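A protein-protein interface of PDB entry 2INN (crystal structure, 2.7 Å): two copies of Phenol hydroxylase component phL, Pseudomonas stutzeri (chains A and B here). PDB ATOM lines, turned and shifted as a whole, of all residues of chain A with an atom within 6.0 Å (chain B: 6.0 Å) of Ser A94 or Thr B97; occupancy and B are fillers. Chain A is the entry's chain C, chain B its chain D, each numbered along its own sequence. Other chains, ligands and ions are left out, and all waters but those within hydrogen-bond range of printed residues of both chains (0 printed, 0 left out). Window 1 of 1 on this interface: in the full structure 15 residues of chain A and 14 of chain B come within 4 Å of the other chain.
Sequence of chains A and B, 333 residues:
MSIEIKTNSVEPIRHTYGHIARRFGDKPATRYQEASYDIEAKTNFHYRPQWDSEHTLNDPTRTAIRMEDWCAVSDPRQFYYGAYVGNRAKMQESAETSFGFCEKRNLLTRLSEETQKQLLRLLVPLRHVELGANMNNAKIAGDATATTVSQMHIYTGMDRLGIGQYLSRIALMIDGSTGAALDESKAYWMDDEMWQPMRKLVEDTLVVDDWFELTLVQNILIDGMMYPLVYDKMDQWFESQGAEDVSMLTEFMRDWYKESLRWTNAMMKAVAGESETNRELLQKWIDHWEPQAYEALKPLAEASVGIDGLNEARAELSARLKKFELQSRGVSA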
ATOM      1  N   ALA A  89       8.534  24.746  12.529  1.00  0.00           N
ATOM      2  CA  ALA A  89       7.845  25.988  12.173  1.00  0.00           C
ATOM      3  C   ALA A  89       6.401  25.679  12.208  1.00  0.00           C
ATOM      4  O   ALA A  89       5.636  26.442  12.792  1.00  0.00           O
ATOM      5  CB  ALA A  89       8.252  26.503  10.826  1.00  0.00           C
ATOM      6  N   LYS A  90       6.027  24.528  11.655  1.00  0.00           N
ATOM      7  CA  LYS A  90       4.615  24.163  11.575  1.00  0.00           C
ATOM      8  C   LYS A  90       4.018  23.940  12.957  1.00  0.00           C
ATOM      9  O   LYS A  90       2.911  24.419  13.244  1.00  0.00           O
ATOM     10  CB  LYS A  90       4.324  22.963  10.667  1.00  0.00           C
ATOM     11  CG  LYS A  90       2.851  22.802  10.515  1.00  0.00           C
ATOM     12  CD  LYS A  90       2.406  21.541   9.901  1.00  0.00           C
ATOM     13  CE  LYS A  90       0.927  21.375  10.246  1.00  0.00           C
ATOM     14  NZ  LYS A  90       0.406  20.228   9.389  1.00  0.00           N
ATOM     15  N   MET A  91       4.758  23.272  13.816  1.00  0.00           N
ATOM     16  CA  MET A  91       4.304  23.020  15.151  1.00  0.00           C
ATOM     17  C   MET A  91       4.115  24.297  16.053  1.00  0.00           C
ATOM     18  O   MET A  91       3.139  24.392  16.853  1.00  0.00           O
ATOM     19  CB  MET A  91       5.335  22.131  15.783  1.00  0.00           C
ATOM     20  CG  MET A  91       4.925  20.687  15.706  1.00  0.00           C
ATOM     21  SD  MET A  91       6.435  19.624  16.384  1.00  0.00           S
ATOM     22  CE  MET A  91       6.188  19.468  18.353  1.00  0.00           C
ATOM     23  N   GLN A  92       5.055  25.250  15.915  1.00  0.00           N
ATOM     24  CA  GLN A  92       5.095  26.390  16.728  1.00  0.00           C
ATOM     25  C   GLN A  92       3.978  27.276  16.328  1.00  0.00           C
ATOM     26  O   GLN A  92       3.293  27.859  17.204  1.00  0.00           O
ATOM     27  CB  GLN A  92       6.466  27.081  16.695  1.00  0.00           C
ATOM     28  CG  GLN A  92       6.880  27.991  15.538  1.00  0.00           C
ATOM     29  CD  GLN A  92       5.948  29.129  15.282  1.00  0.00           C
ATOM     30  OE1 GLN A  92       5.192  29.496  16.136  1.00  0.00           O
ATOM     31  NE2 GLN A  92       5.991  29.688  14.087  1.00  0.00           N
ATOM     32  N   GLU A  93       3.743  27.367  15.019  1.00  0.00           N
ATOM     33  CA  GLU A  93       2.532  28.067  14.557  1.00  0.00           C
ATOM     34  C   GLU A  93       1.292  27.642  15.291  1.00  0.00           C
ATOM     35  O   GLU A  93       0.481  28.433  15.670  1.00  0.00           O
ATOM     36  CB  GLU A  93       2.269  27.815  13.058  1.00  0.00           C
ATOM     37  CG  GLU A  93       1.871  29.032  12.276  1.00  0.00           C
ATOM     38  CD  GLU A  93       2.286  30.268  12.992  1.00  0.00           C
ATOM     39  OE1 GLU A  93       1.574  30.491  14.039  1.00  0.00           O
ATOM     40  OE2 GLU A  93       3.294  30.972  12.561  1.00  0.00           O
ATOM     41  N   SER A  94       1.135  26.358  15.420  1.00  0.00           N
ATOM     42  CA  SER A  94      -0.041  25.772  15.982  1.00  0.00           C
ATOM     43  C   SER A  94      -0.141  26.050  17.474  1.00  0.00           C
ATOM     44  O   SER A  94      -1.188  26.181  17.983  1.00  0.00           O
ATOM     45  CB  SER A  94       0.080  24.273  15.802  1.00  0.00           C
ATOM     46  OG  SER A  94      -1.177  23.727  15.704  1.00  0.00           O
ATOM     47  N   ALA A  95       0.966  26.110  18.183  1.00  0.00           N
ATOM     48  CA  ALA A  95       0.882  26.313  19.579  1.00  0.00           C
ATOM     49  C   ALA A  95       0.615  27.781  19.736  1.00  0.00           C
ATOM     50  O   ALA A  95      -0.109  28.187  20.637  1.00  0.00           O
ATOM     51  CB  ALA A  95       2.211  25.866  20.272  1.00  0.00           C
ATOM     52  N   GLU A  96       1.190  28.572  18.832  1.00  0.00           N
ATOM     53  CA  GLU A  96       1.035  30.016  18.885  1.00  0.00           C
ATOM     54  C   GLU A  96      -0.433  30.385  18.821  1.00  0.00           C
ATOM     55  O   GLU A  96      -0.877  31.403  19.416  1.00  0.00           O
ATOM     56  CB  GLU A  96       1.755  30.758  17.802  1.00  0.00           C
ATOM     57  CG  GLU A  96       1.687  32.248  18.140  1.00  0.00           C
ATOM     58  CD  GLU A  96       2.537  32.580  19.450  1.00  0.00           C
ATOM     59  OE1 GLU A  96       3.663  31.924  19.721  1.00  0.00           O
ATOM     60  OE2 GLU A  96       2.031  33.495  20.195  1.00  0.00           O
ATOM     61  N   THR A  97      -1.173  29.525  18.110  1.00  0.00           N
ATOM     62  CA  THR A  97      -2.647  29.653  18.019  1.00  0.00           C
ATOM     63  C   THR A  97      -3.283  29.449  19.369  1.00  0.00           C
ATOM     64  O   THR A  97      -3.971  30.296  19.850  1.00  0.00           O
ATOM     65  CB  THR A  97      -3.290  28.749  16.858  1.00  0.00           C
ATOM     66  OG1 THR A  97      -3.066  29.411  15.601  1.00  0.00           O
ATOM     67  CG2 THR A  97      -4.782  28.546  17.047  1.00  0.00           C
ATOM     68  N   SER A  98      -2.967  28.320  19.969  1.00  0.00           N
ATOM     69  CA  SER A  98      -3.341  27.934  21.303  1.00  0.00           C
ATOM     70  C   SER A  98      -3.172  29.015  22.373  1.00  0.00           C
ATOM     71  O   SER A  98      -4.095  29.332  23.112  1.00  0.00           O
ATOM     72  CB  SER A  98      -2.415  26.806  21.653  1.00  0.00           C
ATOM     73  OG  SER A  98      -2.618  25.828  20.708  1.00  0.00           O
ATOM     74  N   PHE A  99      -1.954  29.532  22.453  1.00  0.00           N
ATOM     75  CA  PHE A  99      -1.623  30.502  23.434  1.00  0.00           C
ATOM     76  C   PHE A  99      -2.354  31.821  23.198  1.00  0.00           C
ATOM     77  O   PHE A  99      -2.584  32.526  24.152  1.00  0.00           O
ATOM     78  CB  PHE A  99      -0.116  30.715  23.435  1.00  0.00           C
ATOM     79  CG  PHE A  99       0.627  29.769  24.339  1.00  0.00           C
ATOM     80  CD1 PHE A  99       1.005  28.514  23.907  1.00  0.00           C
ATOM     81  CD2 PHE A  99       0.957  30.127  25.615  1.00  0.00           C
ATOM     82  CE1 PHE A  99       1.704  27.651  24.734  1.00  0.00           C
ATOM     83  CE2 PHE A  99       1.655  29.251  26.446  1.00  0.00           C
ATOM     84  CZ  PHE A  99       2.026  28.023  25.995  1.00  0.00           C
ATOM     85  N   GLN B  92      -6.134  29.142   7.770  1.00  0.00           N
ATOM     86  CA  GLN B  92      -6.843  27.877   7.784  1.00  0.00           C
ATOM     87  C   GLN B  92      -6.109  26.833   8.632  1.00  0.00           C
ATOM     88  O   GLN B  92      -6.740  25.866   9.059  1.00  0.00           O
ATOM     89  CB  GLN B  92      -7.056  27.401   6.354  1.00  0.00           C
ATOM     90  CG  GLN B  92      -5.762  27.060   5.636  1.00  0.00           C
ATOM     91  CD  GLN B  92      -5.266  25.651   5.944  1.00  0.00           C
ATOM     92  OE1 GLN B  92      -6.048  24.739   6.155  1.00  0.00           O
ATOM     93  NE2 GLN B  92      -3.976  25.485   5.966  1.00  0.00           N
ATOM     94  N   GLU B  93      -4.787  27.019   8.783  1.00  0.00           N
ATOM     95  CA  GLU B  93      -3.968  26.262   9.709  1.00  0.00           C
ATOM     96  C   GLU B  93      -4.407  26.487  11.130  1.00  0.00           C
ATOM     97  O   GLU B  93      -4.508  25.499  11.857  1.00  0.00           O
ATOM     98  CB  GLU B  93      -2.454  26.574   9.658  1.00  0.00           C
ATOM     99  CG  GLU B  93      -1.564  25.875   8.640  1.00  0.00           C
ATOM    100  CD  GLU B  93      -1.802  24.335   8.568  1.00  0.00           C
ATOM    101  OE1 GLU B  93      -2.182  23.747   9.663  1.00  0.00           O
ATOM    102  OE2 GLU B  93      -1.626  23.757   7.427  1.00  0.00           O
ATOM    103  N   SER B  94      -4.619  27.730  11.573  1.00  0.00           N
ATOM    104  CA  SER B  94      -5.054  27.899  12.953  1.00  0.00           C
ATOM    105  C   SER B  94      -6.339  27.202  13.086  1.00  0.00           C
ATOM    106  O   SER B  94      -6.630  26.562  14.096  1.00  0.00           O
ATOM    107  CB  SER B  94      -5.393  29.307  13.329  1.00  0.00           C
ATOM    108  OG  SER B  94      -4.369  30.137  12.935  1.00  0.00           O
ATOM    109  N   ALA B  95      -7.151  27.300  12.071  1.00  0.00           N
ATOM    110  CA  ALA B  95      -8.442  26.698  12.282  1.00  0.00           C
ATOM    111  C   ALA B  95      -8.193  25.203  12.472  1.00  0.00           C
ATOM    112  O   ALA B  95      -8.836  24.609  13.356  1.00  0.00           O
ATOM    113  CB  ALA B  95      -9.448  27.017  11.155  1.00  0.00           C
ATOM    114  N   GLU B  96      -7.240  24.628  11.717  1.00  0.00           N
ATOM    115  CA  GLU B  96      -7.102  23.169  11.715  1.00  0.00           C
ATOM    116  C   GLU B  96      -6.667  22.746  13.071  1.00  0.00           C
ATOM    117  O   GLU B  96      -7.201  21.745  13.575  1.00  0.00           O
ATOM    118  CB  GLU B  96      -6.123  22.585  10.681  1.00  0.00           C
ATOM    119  CG  GLU B  96      -6.839  22.117   9.434  1.00  0.00           C
ATOM    120  CD  GLU B  96      -7.867  21.047   9.710  1.00  0.00           C
ATOM    121  OE1 GLU B  96      -7.541  20.112  10.504  1.00  0.00           O
ATOM    122  OE2 GLU B  96      -8.990  21.156   9.120  1.00  0.00           O
ATOM    123  N   THR B  97      -5.751  23.535  13.660  1.00  0.00           N
ATOM    124  CA  THR B  97      -5.378  23.285  15.047  1.00  0.00           C
ATOM    125  C   THR B  97      -6.601  23.176  15.996  1.00  0.00           C
ATOM    126  O   THR B  97      -6.738  22.150  16.760  1.00  0.00           O
ATOM    127  CB  THR B  97      -4.550  24.375  15.600  1.00  0.00           C
ATOM    128  OG1 THR B  97      -3.423  24.581  14.730  1.00  0.00           O
ATOM    129  CG2 THR B  97      -4.142  24.094  17.118  1.00  0.00           C
ATOM    130  N   SER B  98      -7.485  24.190  15.907  1.00  0.00           N
ATOM    131  CA  SER B  98      -8.609  24.231  16.780  1.00  0.00           C
ATOM    132  C   SER B  98      -9.491  23.081  16.463  1.00  0.00           C
ATOM    133  O   SER B  98      -9.931  22.449  17.394  1.00  0.00           O
ATOM    134  CB  SER B  98      -9.389  25.480  16.571  1.00  0.00           C
ATOM    135  OG  SER B  98      -8.535  26.569  16.622  1.00  0.00           O
ATOM    136  N   PHE B  99      -9.793  22.784  15.193  1.00  0.00           N
ATOM    137  CA  PHE B  99     -10.629  21.628  14.968  1.00  0.00           C
ATOM    138  C   PHE B  99     -10.059  20.244  15.424  1.00  0.00           C
ATOM    139  O   PHE B  99     -10.789  19.419  15.955  1.00  0.00           O
ATOM    140  CB  PHE B  99     -11.017  21.511  13.521  1.00  0.00           C
ATOM    141  CG  PHE B  99     -12.036  22.483  13.123  1.00  0.00           C
ATOM    142  CD1 PHE B  99     -11.706  23.815  12.947  1.00  0.00           C
ATOM    143  CD2 PHE B  99     -13.350  22.083  12.963  1.00  0.00           C
ATOM    144  CE1 PHE B  99     -12.709  24.740  12.587  1.00  0.00           C
ATOM    145  CE2 PHE B  99     -14.345  22.986  12.615  1.00  0.00           C
ATOM    146  CZ  PHE B  99     -14.019  24.315  12.416  1.00  0.00           C
ATOM    147  N   GLY B 100      -8.763  20.001  15.240  1.00  0.00           N
ATOM    148  CA  GLY B 100      -8.186  18.750  15.715  1.00  0.00           C
ATOM    149  C   GLY B 100      -8.544  18.652  17.194  1.00  0.00           C
ATOM    150  O   GLY B 100      -9.227  17.697  17.607  1.00  0.00           O
ATOM    151  N   PHE B 101      -8.129  19.680  17.952  1.00  0.00           N
ATOM    152  CA  PHE B 101      -8.287  19.777  19.404  1.00  0.00           C
ATOM    153  C   PHE B 101      -9.716  19.624  19.882  1.00  0.00           C
ATOM    154  O   PHE B 101      -9.895  18.902  20.849  1.00  0.00           O
ATOM    155  CB  PHE B 101      -7.702  21.060  19.962  1.00  0.00           C
ATOM    156  CG  PHE B 101      -7.498  21.013  21.417  1.00  0.00           C
ATOM    157  CD1 PHE B 101      -6.378  20.450  21.947  1.00  0.00           C
ATOM    158  CD2 PHE B 101      -8.457  21.489  22.286  1.00  0.00           C
ATOM    159  CE1 PHE B 101      -6.245  20.341  23.361  1.00  0.00           C
ATOM    160  CE2 PHE B 101      -8.302  21.424  23.699  1.00  0.00           C
ATOM    161  CZ  PHE B 101      -7.212  20.853  24.224  1.00  0.00           C
ATOM    162  N   CYS B 102     -10.733  20.202  19.205  1.00  0.00           N
ATOM    163  CA  CYS B 102     -12.135  20.010  19.687  1.00  0.00           C
ATOM    164  C   CYS B 102     -12.611  18.568  19.570  1.00  0.00           C
ATOM    165  O   CYS B 102     -13.698  18.193  20.118  1.00  0.00           O
ATOM    166  CB  CYS B 102     -13.179  20.982  19.094  1.00  0.00           C
ATOM    167  SG  CYS B 102     -12.628  22.620  19.607  1.00  0.00           S
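Ser A94 touches Thr B97, and with the chains exchanged Thr A97 touches Ser B94.
Of the 3 pairs that touch across the chains among the printed residues, 2 have their exchanged pair printed and touching as well.
The backbone carbonyl oxygen (O) of Glu B93 is in hydrogen-bond range of the side-chain hydroxyl (OG1) of Thr B97 (3.2 Å).
The side-chain hydroxyl (OG) of Ser B98 is in hydrogen-bond range of the backbone carbonyl oxygen (O) of Ser B94.
O of Ser A94 sits at hydrogen-bond distance from OG of Ser A98.
The side-chain amide nitrogen of Gln B92 is in hydrogen-bond range of the side-chain carboxylate of Glu B93.
Printed residues of chain B within 4 Å of Ser A94: Thr B97 (2.6 Å).
Of the printed residues of chain A, Thr B97 touches Ser A94 (2.6 Å).
Of the printed residues of chain A, Glu B93 touches Lys A90 (3.95 Å).
Of the printed residues of chain B, Thr A97 touches Ser B94.
Of the printed residues of chain A, Ser B94 touches Thr A97 (3.1 Å).
Ser A98 touches none of the printed residues of chain B.
The nearest residue of chain B that does not touch Ser A94 is Glu B93 (5.4 Å).
The nearest residue of chain A that does not touch Thr B97 is Ser A98 (4.3 Å).
The nearest printed residue of chain A that does not touch Ser B94 is Glu A93 (5.8 Å).
OG of Ser A94 is in hydrogen-bond range of OG1 of Thr B97 (2.6 Å).
The side-chain hydroxyl (OG1) of Thr A97 sits at hydrogen-bond distance from the side-chain hydroxyl (OG) of Ser B94 (3.1 Å).
OE1 of Glu B93 touches CE of Lys A90 (3.95 Å).
Of the 11 printed residues of chain B, 3 touch a printed residue of chain A.
Along chain B the printed residues that touch a printed residue of chain A span positions 93 to 97.
Among the printed residues, 3 pairs touch across the chains.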
